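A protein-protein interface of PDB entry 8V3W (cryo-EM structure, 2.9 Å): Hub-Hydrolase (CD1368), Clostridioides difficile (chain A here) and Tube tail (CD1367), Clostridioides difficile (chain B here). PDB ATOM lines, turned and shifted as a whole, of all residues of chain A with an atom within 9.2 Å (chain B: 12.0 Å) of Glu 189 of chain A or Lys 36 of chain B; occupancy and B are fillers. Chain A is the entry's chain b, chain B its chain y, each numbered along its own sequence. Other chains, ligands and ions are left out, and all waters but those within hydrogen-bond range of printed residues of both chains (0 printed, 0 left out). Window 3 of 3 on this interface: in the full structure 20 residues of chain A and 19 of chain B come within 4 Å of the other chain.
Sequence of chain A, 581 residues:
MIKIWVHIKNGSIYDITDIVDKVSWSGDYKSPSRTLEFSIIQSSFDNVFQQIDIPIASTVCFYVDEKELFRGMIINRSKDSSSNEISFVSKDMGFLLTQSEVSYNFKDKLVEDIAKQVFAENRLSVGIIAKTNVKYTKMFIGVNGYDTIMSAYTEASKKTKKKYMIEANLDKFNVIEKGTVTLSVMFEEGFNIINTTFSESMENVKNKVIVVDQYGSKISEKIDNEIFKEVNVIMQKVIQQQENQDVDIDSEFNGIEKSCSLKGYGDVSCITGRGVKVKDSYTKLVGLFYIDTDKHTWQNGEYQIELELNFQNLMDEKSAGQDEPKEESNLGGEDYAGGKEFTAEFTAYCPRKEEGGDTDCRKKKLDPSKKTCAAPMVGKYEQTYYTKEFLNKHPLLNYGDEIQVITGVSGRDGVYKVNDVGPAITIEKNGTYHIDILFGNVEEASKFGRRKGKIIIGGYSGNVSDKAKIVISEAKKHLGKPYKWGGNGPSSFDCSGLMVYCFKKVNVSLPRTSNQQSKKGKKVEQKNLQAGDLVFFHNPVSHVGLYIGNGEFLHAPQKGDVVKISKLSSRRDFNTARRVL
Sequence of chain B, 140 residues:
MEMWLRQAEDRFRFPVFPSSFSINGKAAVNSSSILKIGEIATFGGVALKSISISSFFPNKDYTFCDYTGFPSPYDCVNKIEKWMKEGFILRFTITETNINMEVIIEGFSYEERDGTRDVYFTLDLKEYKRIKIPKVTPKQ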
ATOM      1  N   MET A 186       9.041  18.693  -4.351  1.00  0.00           N
ATOM      2  CA  MET A 186       7.984  19.076  -3.429  1.00  0.00           C
ATOM      3  C   MET A 186       8.410  18.711  -2.017  1.00  0.00           C
ATOM      4  O   MET A 186       8.993  17.648  -1.793  1.00  0.00           O
ATOM      5  CB  MET A 186       6.660  18.379  -3.774  1.00  0.00           C
ATOM      6  CG  MET A 186       5.701  18.261  -2.601  1.00  0.00           C
ATOM      7  SD  MET A 186       4.093  17.543  -2.975  1.00  0.00           S
ATOM      8  CE  MET A 186       3.941  17.918  -4.713  1.00  0.00           C
ATOM      9  N   PHE A 187       8.128  19.593  -1.065  1.00  0.00           N
ATOM     10  CA  PHE A 187       8.474  19.358   0.328  1.00  0.00           C
ATOM     11  C   PHE A 187       7.305  18.681   1.034  1.00  0.00           C
ATOM     12  O   PHE A 187       6.181  19.190   1.010  1.00  0.00           O
ATOM     13  CB  PHE A 187       8.846  20.670   1.014  1.00  0.00           C
ATOM     14  CG  PHE A 187      10.192  21.195   0.613  1.00  0.00           C
ATOM     15  CD1 PHE A 187      11.340  20.698   1.194  1.00  0.00           C
ATOM     16  CD2 PHE A 187      10.309  22.173  -0.355  1.00  0.00           C
ATOM     17  CE1 PHE A 187      12.575  21.168   0.823  1.00  0.00           C
ATOM     18  CE2 PHE A 187      11.542  22.644  -0.729  1.00  0.00           C
ATOM     19  CZ  PHE A 187      12.677  22.142  -0.141  1.00  0.00           C
ATOM     20  N   GLU A 188       7.570  17.531   1.650  1.00  0.00           N
ATOM     21  CA  GLU A 188       6.575  16.789   2.407  1.00  0.00           C
ATOM     22  C   GLU A 188       7.107  16.512   3.803  1.00  0.00           C
ATOM     23  O   GLU A 188       8.315  16.384   4.008  1.00  0.00           O
ATOM     24  CB  GLU A 188       6.210  15.464   1.738  1.00  0.00           C
ATOM     25  CG  GLU A 188       6.086  15.530   0.236  1.00  0.00           C
ATOM     26  CD  GLU A 188       5.162  14.464  -0.316  1.00  0.00           C
ATOM     27  OE1 GLU A 188       5.020  13.405   0.326  1.00  0.00           O
ATOM     28  OE2 GLU A 188       4.583  14.686  -1.397  1.00  0.00           O
ATOM     29  N   GLU A 189       6.184  16.409   4.758  1.00  0.00           N
ATOM     30  CA  GLU A 189       6.574  16.262   6.156  1.00  0.00           C
ATOM     31  C   GLU A 189       7.329  14.962   6.393  1.00  0.00           C
ATOM     32  O   GLU A 189       8.339  14.947   7.103  1.00  0.00           O
ATOM     33  CB  GLU A 189       5.342  16.337   7.054  1.00  0.00           C
ATOM     34  CG  GLU A 189       5.653  16.723   8.483  1.00  0.00           C
ATOM     35  CD  GLU A 189       4.593  17.612   9.100  1.00  0.00           C
ATOM     36  OE1 GLU A 189       3.913  18.338   8.350  1.00  0.00           O
ATOM     37  OE2 GLU A 189       4.443  17.589  10.338  1.00  0.00           O
ATOM     38  N   GLY A 190       6.871  13.869   5.803  1.00  0.00           N
ATOM     39  CA  GLY A 190       7.501  12.594   6.062  1.00  0.00           C
ATOM     40  C   GLY A 190       8.721  12.265   5.237  1.00  0.00           C
ATOM     41  O   GLY A 190       9.245  11.155   5.355  1.00  0.00           O
ATOM     42  N   PHE A 191       9.186  13.175   4.379  1.00  0.00           N
ATOM     43  CA  PHE A 191      10.262  12.853   3.447  1.00  0.00           C
ATOM     44  C   PHE A 191      11.499  13.725   3.622  1.00  0.00           C
ATOM     45  O   PHE A 191      12.576  13.193   3.903  1.00  0.00           O
ATOM     46  CB  PHE A 191       9.733  12.951   2.014  1.00  0.00           C
ATOM     47  CG  PHE A 191       8.831  11.821   1.622  1.00  0.00           C
ATOM     48  CD1 PHE A 191       7.562  11.710   2.161  1.00  0.00           C
ATOM     49  CD2 PHE A 191       9.248  10.870   0.711  1.00  0.00           C
ATOM     50  CE1 PHE A 191       6.731  10.673   1.804  1.00  0.00           C
ATOM     51  CE2 PHE A 191       8.419   9.832   0.345  1.00  0.00           C
ATOM     52  CZ  PHE A 191       7.160   9.734   0.895  1.00  0.00           C
ATOM     53  N   ASN A 192      11.393  15.048   3.469  1.00  0.00           N
ATOM     54  CA  ASN A 192      12.602  15.861   3.387  1.00  0.00           C
ATOM     55  C   ASN A 192      12.486  17.185   4.134  1.00  0.00           C
ATOM     56  O   ASN A 192      13.131  18.165   3.755  1.00  0.00           O
ATOM     57  CB  ASN A 192      12.979  16.134   1.929  1.00  0.00           C
ATOM     58  CG  ASN A 192      11.858  16.781   1.147  1.00  0.00           C
ATOM     59  OD1 ASN A 192      10.788  17.046   1.680  1.00  0.00           O
ATOM     60  ND2 ASN A 192      12.105  17.049  -0.124  1.00  0.00           N
ATOM     61  N   ILE A 193      11.690  17.246   5.194  1.00  0.00           N
ATOM     62  CA  ILE A 193      11.520  18.468   5.970  1.00  0.00           C
ATOM     63  C   ILE A 193      12.117  18.256   7.353  1.00  0.00           C
ATOM     64  O   ILE A 193      11.783  17.283   8.037  1.00  0.00           O
ATOM     65  CB  ILE A 193      10.043  18.882   6.067  1.00  0.00           C
ATOM     66  CG1 ILE A 193       9.553  19.412   4.724  1.00  0.00           C
ATOM     67  CG2 ILE A 193       9.856  19.939   7.128  1.00  0.00           C
ATOM     68  CD1 ILE A 193       8.087  19.750   4.710  1.00  0.00           C
ATOM     69  N   ILE A 194      13.003  19.158   7.759  1.00  0.00           N
ATOM     70  CA  ILE A 194      13.542  19.132   9.112  1.00  0.00           C
ATOM     71  C   ILE A 194      12.626  19.860  10.084  1.00  0.00           C
ATOM     72  O   ILE A 194      12.284  19.331  11.143  1.00  0.00           O
ATOM     73  CB  ILE A 194      14.966  19.724   9.131  1.00  0.00           C
ATOM     74  CG1 ILE A 194      15.914  18.853   8.309  1.00  0.00           C
ATOM     75  CG2 ILE A 194      15.471  19.839  10.552  1.00  0.00           C
ATOM     76  CD1 ILE A 194      17.252  19.488   8.055  1.00  0.00           C
ATOM     77  N   ASN A 195      12.201  21.073   9.738  1.00  0.00           N
ATOM     78  CA  ASN A 195      11.299  21.833  10.590  1.00  0.00           C
ATOM     79  C   ASN A 195      10.619  22.908   9.758  1.00  0.00           C
ATOM     80  O   ASN A 195      11.124  23.314   8.711  1.00  0.00           O
ATOM     81  CB  ASN A 195      12.042  22.454  11.775  1.00  0.00           C
ATOM     82  CG  ASN A 195      11.146  22.673  12.975  1.00  0.00           C
ATOM     83  OD1 ASN A 195      10.204  21.918  13.205  1.00  0.00           O
ATOM     84  ND2 ASN A 195      11.431  23.714  13.744  1.00  0.00           N
ATOM     85  N   THR A 196       9.463  23.364  10.239  1.00  0.00           N
ATOM     86  CA  THR A 196       8.725  24.451   9.611  1.00  0.00           C
ATOM     87  C   THR A 196       8.084  25.318  10.684  1.00  0.00           C
ATOM     88  O   THR A 196       7.853  24.877  11.810  1.00  0.00           O
ATOM     89  CB  THR A 196       7.635  23.942   8.660  1.00  0.00           C
ATOM     90  OG1 THR A 196       6.997  22.798   9.233  1.00  0.00           O
ATOM     91  CG2 THR A 196       8.221  23.565   7.317  1.00  0.00           C
ATOM     92  N   PHE A 198       4.834  28.195  10.555  1.00  0.00           N
ATOM     93  CA  PHE A 198       3.828  28.931   9.804  1.00  0.00           C
ATOM     94  C   PHE A 198       3.320  30.107  10.623  1.00  0.00           C
ATOM     95  O   PHE A 198       3.145  29.998  11.839  1.00  0.00           O
ATOM     96  CB  PHE A 198       2.661  28.024   9.425  1.00  0.00           C
ATOM     97  CG  PHE A 198       3.051  26.865   8.567  1.00  0.00           C
ATOM     98  CD1 PHE A 198       3.159  27.005   7.198  1.00  0.00           C
ATOM     99  CD2 PHE A 198       3.307  25.632   9.129  1.00  0.00           C
ATOM    100  CE1 PHE A 198       3.513  25.937   6.409  1.00  0.00           C
ATOM    101  CE2 PHE A 198       3.664  24.565   8.344  1.00  0.00           C
ATOM    102  CZ  PHE A 198       3.770  24.718   6.984  1.00  0.00           C
ATOM    103  N   LEU A 262      11.123  27.426   6.380  1.00  0.00           N
ATOM    104  CA  LEU A 262      11.355  26.009   6.140  1.00  0.00           C
ATOM    105  C   LEU A 262      12.845  25.696   6.132  1.00  0.00           C
ATOM    106  O   LEU A 262      13.648  26.463   5.597  1.00  0.00           O
ATOM    107  CB  LEU A 262      10.720  25.583   4.814  1.00  0.00           C
ATOM    108  CG  LEU A 262      10.690  24.102   4.444  1.00  0.00           C
ATOM    109  CD1 LEU A 262       9.398  23.780   3.733  1.00  0.00           C
ATOM    110  CD2 LEU A 262      11.866  23.745   3.568  1.00  0.00           C
ATOM    111  N   LYS A 263      13.204  24.563   6.728  1.00  0.00           N
ATOM    112  CA  LYS A 263      14.558  24.028   6.677  1.00  0.00           C
ATOM    113  C   LYS A 263      14.485  22.556   6.301  1.00  0.00           C
ATOM    114  O   LYS A 263      13.732  21.799   6.917  1.00  0.00           O
ATOM    115  CB  LYS A 263      15.271  24.206   8.017  1.00  0.00           C
ATOM    116  CG  LYS A 263      16.609  23.523   8.103  1.00  0.00           C
ATOM    117  CD  LYS A 263      17.454  24.148   9.190  1.00  0.00           C
ATOM    118  CE  LYS A 263      18.600  23.242   9.586  1.00  0.00           C
ATOM    119  NZ  LYS A 263      18.200  22.256  10.622  1.00  0.00           N
ATOM    120  N   LYS A 277       6.378  23.991  -3.908  1.00  0.00           N
ATOM    121  CA  LYS A 277       5.161  23.339  -3.438  1.00  0.00           C
ATOM    122  C   LYS A 277       5.407  22.658  -2.100  1.00  0.00           C
ATOM    123  O   LYS A 277       6.402  21.949  -1.934  1.00  0.00           O
ATOM    124  CB  LYS A 277       4.664  22.322  -4.464  1.00  0.00           C
ATOM    125  CG  LYS A 277       3.831  22.947  -5.553  1.00  0.00           C
ATOM    126  CD  LYS A 277       4.117  22.339  -6.909  1.00  0.00           C
ATOM    127  CE  LYS A 277       3.831  20.863  -6.930  1.00  0.00           C
ATOM    128  NZ  LYS A 277       4.302  20.262  -8.197  1.00  0.00           N
ATOM    129  N   VAL A 278       4.500  22.878  -1.151  1.00  0.00           N
ATOM    130  CA  VAL A 278       4.558  22.267   0.172  1.00  0.00           C
ATOM    131  C   VAL A 278       3.238  21.559   0.429  1.00  0.00           C
ATOM    132  O   VAL A 278       2.169  22.131   0.197  1.00  0.00           O
ATOM    133  CB  VAL A 278       4.837  23.304   1.278  1.00  0.00           C
ATOM    134  CG1 VAL A 278       5.258  22.611   2.551  1.00  0.00           C
ATOM    135  CG2 VAL A 278       5.903  24.288   0.834  1.00  0.00           C
ATOM    136  N   LYS A 279       3.310  20.323   0.912  1.00  0.00           N
ATOM    137  CA  LYS A 279       2.134  19.503   1.166  1.00  0.00           C
ATOM    138  C   LYS A 279       1.740  19.586   2.633  1.00  0.00           C
ATOM    139  O   LYS A 279       2.591  19.460   3.517  1.00  0.00           O
ATOM    140  CB  LYS A 279       2.393  18.049   0.784  1.00  0.00           C
ATOM    141  CG  LYS A 279       1.142  17.210   0.681  1.00  0.00           C
ATOM    142  CD  LYS A 279       1.450  15.749   0.919  1.00  0.00           C
ATOM    143  CE  LYS A 279       0.713  14.868  -0.069  1.00  0.00           C
ATOM    144  NZ  LYS A 279       1.294  14.977  -1.433  1.00  0.00           N
ATOM    145  N   ASP A 280       0.451  19.790   2.884  1.00  0.00           N
ATOM    146  CA  ASP A 280      -0.065  19.823   4.245  1.00  0.00           C
ATOM    147  C   ASP A 280      -0.273  18.406   4.756  1.00  0.00           C
ATOM    148  O   ASP A 280      -0.819  17.555   4.050  1.00  0.00           O
ATOM    149  CB  ASP A 280      -1.372  20.608   4.294  1.00  0.00           C
ATOM    150  CG  ASP A 280      -1.963  20.666   5.679  1.00  0.00           C
ATOM    151  OD1 ASP A 280      -1.203  20.563   6.661  1.00  0.00           O
ATOM    152  OD2 ASP A 280      -3.193  20.815   5.790  1.00  0.00           O
ATOM    153  N   SER A 281       0.165  18.152   5.989  1.00  0.00           N
ATOM    154  CA  SER A 281       0.149  16.788   6.509  1.00  0.00           C
ATOM    155  C   SER A 281      -1.255  16.340   6.898  1.00  0.00           C
ATOM    156  O   SER A 281      -1.645  15.201   6.614  1.00  0.00           O
ATOM    157  CB  SER A 281       1.102  16.673   7.697  1.00  0.00           C
ATOM    158  OG  SER A 281       1.122  17.870   8.450  1.00  0.00           O
ATOM    159  N   TYR A 282      -2.027  17.206   7.557  1.00  0.00           N
ATOM    160  CA  TYR A 282      -3.321  16.776   8.081  1.00  0.00           C
ATOM    161  C   TYR A 282      -4.348  16.582   6.971  1.00  0.00           C
ATOM    162  O   TYR A 282      -5.047  15.564   6.934  1.00  0.00           O
ATOM    163  CB  TYR A 282      -3.831  17.779   9.114  1.00  0.00           C
ATOM    164  CG  TYR A 282      -5.200  17.443   9.661  1.00  0.00           C
ATOM    165  CD1 TYR A 282      -5.364  16.453  10.617  1.00  0.00           C
ATOM    166  CD2 TYR A 282      -6.327  18.117   9.221  1.00  0.00           C
ATOM    167  CE1 TYR A 282      -6.611  16.145  11.116  1.00  0.00           C
ATOM    168  CE2 TYR A 282      -7.579  17.816   9.713  1.00  0.00           C
ATOM    169  CZ  TYR A 282      -7.715  16.830  10.660  1.00  0.00           C
ATOM    170  OH  TYR A 282      -8.961  16.529  11.152  1.00  0.00           O
ATOM    171  N   THR A 283      -4.462  17.547   6.059  1.00  0.00           N
ATOM    172  CA  THR A 283      -5.486  17.500   5.023  1.00  0.00           C
ATOM    173  C   THR A 283      -4.992  16.942   3.695  1.00  0.00           C
ATOM    174  O   THR A 283      -5.803  16.775   2.779  1.00  0.00           O
ATOM    175  CB  THR A 283      -6.068  18.895   4.775  1.00  0.00           C
ATOM    176  OG1 THR A 283      -5.111  19.689   4.067  1.00  0.00           O
ATOM    177  CG2 THR A 283      -6.407  19.575   6.080  1.00  0.00           C
ATOM    178  N   LYS A 284      -3.698  16.649   3.570  1.00  0.00           N
ATOM    179  CA  LYS A 284      -3.110  16.169   2.317  1.00  0.00           C
ATOM    180  C   LYS A 284      -3.389  17.127   1.161  1.00  0.00           C
ATOM    181  O   LYS A 284      -3.678  16.712   0.039  1.00  0.00           O
ATOM    182  CB  LYS A 284      -3.597  14.758   1.979  1.00  0.00           C
ATOM    183  CG  LYS A 284      -3.582  13.795   3.145  1.00  0.00           C
ATOM    184  CD  LYS A 284      -2.202  13.683   3.752  1.00  0.00           C
ATOM    185  CE  LYS A 284      -2.153  12.575   4.783  1.00  0.00           C
ATOM    186  NZ  LYS A 284      -2.681  11.301   4.230  1.00  0.00           N
ATOM    187  N   LEU A 285      -3.297  18.424   1.439  1.00  0.00           N
ATOM    188  CA  LEU A 285      -3.472  19.464   0.438  1.00  0.00           C
ATOM    189  C   LEU A 285      -2.131  20.114   0.129  1.00  0.00           C
ATOM    190  O   LEU A 285      -1.264  20.227   0.998  1.00  0.00           O
ATOM    191  CB  LEU A 285      -4.466  20.527   0.910  1.00  0.00           C
ATOM    192  CG  LEU A 285      -5.944  20.136   0.928  1.00  0.00           C
ATOM    193  CD1 LEU A 285      -6.749  21.175   1.679  1.00  0.00           C
ATOM    194  CD2 LEU A 285      -6.474  19.965  -0.483  1.00  0.00           C
ATOM    195  N   SER B  32      20.959  14.362  12.411  1.00  0.00           N
ATOM    196  CA  SER B  32      19.880  15.269  12.057  1.00  0.00           C
ATOM    197  C   SER B  32      18.570  14.578  12.405  1.00  0.00           C
ATOM    198  O   SER B  32      18.551  13.550  13.086  1.00  0.00           O
ATOM    199  CB  SER B  32      19.942  15.657  10.575  1.00  0.00           C
ATOM    200  OG  SER B  32      21.226  16.133  10.223  1.00  0.00           O
ATOM    201  N   SER B  33      17.464  15.144  11.936  1.00  0.00           N
ATOM    202  CA  SER B  33      16.160  14.539  12.144  1.00  0.00           C
ATOM    203  C   SER B  33      15.227  14.997  11.036  1.00  0.00           C
ATOM    204  O   SER B  33      15.443  16.033  10.406  1.00  0.00           O
ATOM    205  CB  SER B  33      15.581  14.902  13.514  1.00  0.00           C
ATOM    206  OG  SER B  33      14.953  16.169  13.470  1.00  0.00           O
ATOM    207  N   ILE B  34      14.184  14.212  10.809  1.00  0.00           N
ATOM    208  CA  ILE B  34      13.158  14.518   9.822  1.00  0.00           C
ATOM    209  C   ILE B  34      11.803  14.363  10.492  1.00  0.00           C
ATOM    210  O   ILE B  34      11.601  13.440  11.286  1.00  0.00           O
ATOM    211  CB  ILE B  34      13.280  13.609   8.583  1.00  0.00           C
ATOM    212  CG1 ILE B  34      14.509  14.001   7.768  1.00  0.00           C
ATOM    213  CG2 ILE B  34      12.037  13.681   7.721  1.00  0.00           C
ATOM    214  CD1 ILE B  34      14.704  13.174   6.537  1.00  0.00           C
ATOM    215  N   LEU B  35      10.887  15.282  10.197  1.00  0.00           N
ATOM    216  CA  LEU B  35       9.560  15.240  10.799  1.00  0.00           C
ATOM    217  C   LEU B  35       8.858  13.928  10.473  1.00  0.00           C
ATOM    218  O   LEU B  35       8.853  13.479   9.324  1.00  0.00           O
ATOM    219  CB  LEU B  35       8.728  16.420  10.309  1.00  0.00           C
ATOM    220  CG  LEU B  35       8.967  17.754  11.013  1.00  0.00           C
ATOM    221  CD1 LEU B  35       8.121  18.842  10.391  1.00  0.00           C
ATOM    222  CD2 LEU B  35       8.677  17.633  12.490  1.00  0.00           C
ATOM    223  N   LYS B  36       8.274  13.310  11.498  1.00  0.00           N
ATOM    224  CA  LYS B  36       7.502  12.071  11.421  1.00  0.00           C
ATOM    225  C   LYS B  36       8.340  10.855  11.053  1.00  0.00           C
ATOM    226  O   LYS B  36       7.773   9.795  10.771  1.00  0.00           O
ATOM    227  CB  LYS B  36       6.334  12.179  10.433  1.00  0.00           C
ATOM    228  CG  LYS B  36       5.467  13.406  10.610  1.00  0.00           C
ATOM    229  CD  LYS B  36       4.911  13.496  12.013  1.00  0.00           C
ATOM    230  CE  LYS B  36       3.815  14.541  12.098  1.00  0.00           C
ATOM    231  NZ  LYS B  36       2.491  13.983  11.711  1.00  0.00           N
ATOM    232  N   ILE B  37       9.665  10.966  11.033  1.00  0.00           N
ATOM    233  CA  ILE B  37      10.502   9.822  10.694  1.00  0.00           C
ATOM    234  C   ILE B  37      11.450   9.518  11.847  1.00  0.00           C
ATOM    235  O   ILE B  37      11.784   8.357  12.100  1.00  0.00           O
ATOM    236  CB  ILE B  37      11.275  10.076   9.386  1.00  0.00           C
ATOM    237  CG1 ILE B  37      10.335   9.974   8.186  1.00  0.00           C
ATOM    238  CG2 ILE B  37      12.448   9.117   9.230  1.00  0.00           C
ATOM    239  CD1 ILE B  37      10.235   8.588   7.601  1.00  0.00           C
ATOM    240  N   GLY B  38      11.848  10.549  12.585  1.00  0.00           N
ATOM    241  CA  GLY B  38      12.823  10.368  13.643  1.00  0.00           C
ATOM    242  C   GLY B  38      14.219  10.817  13.266  1.00  0.00           C
ATOM    243  O   GLY B  38      14.384  11.767  12.499  1.00  0.00           O
ATOM    244  N   GLU B  39      15.232  10.135  13.790  1.00  0.00           N
ATOM    245  CA  GLU B  39      16.625  10.546  13.654  1.00  0.00           C
ATOM    246  C   GLU B  39      17.275   9.922  12.424  1.00  0.00           C
ATOM    247  O   GLU B  39      16.963   8.789  12.051  1.00  0.00           O
ATOM    248  CB  GLU B  39      17.400  10.150  14.912  1.00  0.00           C
ATOM    249  CG  GLU B  39      18.853  10.572  14.930  1.00  0.00           C
ATOM    250  CD  GLU B  39      19.710   9.678  15.805  1.00  0.00           C
ATOM    251  OE1 GLU B  39      19.232   8.600  16.205  1.00  0.00           O
ATOM    252  OE2 GLU B  39      20.867  10.049  16.089  1.00  0.00           O
ATOM    253  N   ILE B  40      18.183  10.675  11.793  1.00  0.00           N
ATOM    254  CA  ILE B  40      19.000  10.190  10.686  1.00  0.00           C
ATOM    255  C   ILE B  40      20.448  10.589  10.934  1.00  0.00           C
ATOM    256  O   ILE B  40      20.747  11.447  11.765  1.00  0.00           O
ATOM    257  CB  ILE B  40      18.531  10.724   9.319  1.00  0.00           C
ATOM    258  CG1 ILE B  40      18.668  12.241   9.281  1.00  0.00           C
ATOM    259  CG2 ILE B  40      17.106  10.294   9.032  1.00  0.00           C
ATOM    260  CD1 ILE B  40      18.394  12.836   7.939  1.00  0.00           C
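O of Glu 189 of chain A sits close to O of Leu 35 of chain B, 2.7 Å away.
O of Ile 193 of chain A sits at hydrogen-bond distance from N of Leu 35 of chain B, 3.1 Å away.
OE1 of Glu 189 of chain A lies within hydrogen-bond range of OG of Ser 281 of chain A, 2.8 Å away.
N of Ile 194 of chain A sits at hydrogen-bond distance from O of Lys 263 of chain A.
Among the printed residues, pairs that only touch across the chains: Gly 190 of chain A with Ile 37 of chain B (3.3 Å), Phe 191 of chain A with Ile 34 of chain B (3.4 Å), Ile 194 of chain A with Ser 33 of chain B (3.5 Å), Ile 193 of chain A with Ile 34 of chain B (3.6 Å), Glu 189 of chain A with Lys 36 of chain B (3.6 Å), Gly 190 of chain A with Leu 35 of chain B (3.6 Å), Ile 194 of chain A with Leu 35 of chain B (3.7 Å) and Glu 189 of chain A with Ile 34 of chain B (3.96 Å).
Of chain B, only Ile 34 (3.96 Å), Leu 35 (2.7 Å) and Lys 36 (3.6 Å) come within 4 Å of Glu 189 of chain A.
Lys 36 of chain B touches just one residue of chain A: Glu 189 (3.6 Å).
Of chain B, only Leu 35 and Ile 37 come within 4 Å of Gly 190 of chain A.
No residue of chain B comes within 4 Å of Asn 192 of chain A.
No residue of chain B comes within 4 Å of Asp 280 of chain A.
No residue of chain B comes within 4 Å of Ser 281 of chain A.
Of the printed residues of chain A, Leu 35 of chain B touches Glu 189, Gly 190, Ile 193 and Ile 194.
Of the printed residues of chain A, Ile 37 of chain B touches Gly 190 (3.3 Å).
Printed residues of chain A within 4 Å of Ile 34 of chain B: Glu 189, Phe 191 and Ile 193.
Printed residues of chain B within 4 Å of Ile 194 of chain A: Ser 33 and Leu 35.
The nearest printed residue of chain A that does not touch Ser 33 of chain B is Ile 193 of chain A (4.5 Å).
Printed residues of chain B that touch a printed residue of chain A: Ser 33, Ile 34, Leu 35, Lys 36 and Ile 37.
Of the 23 printed residues of chain A, 5 touch a printed residue of chain B.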
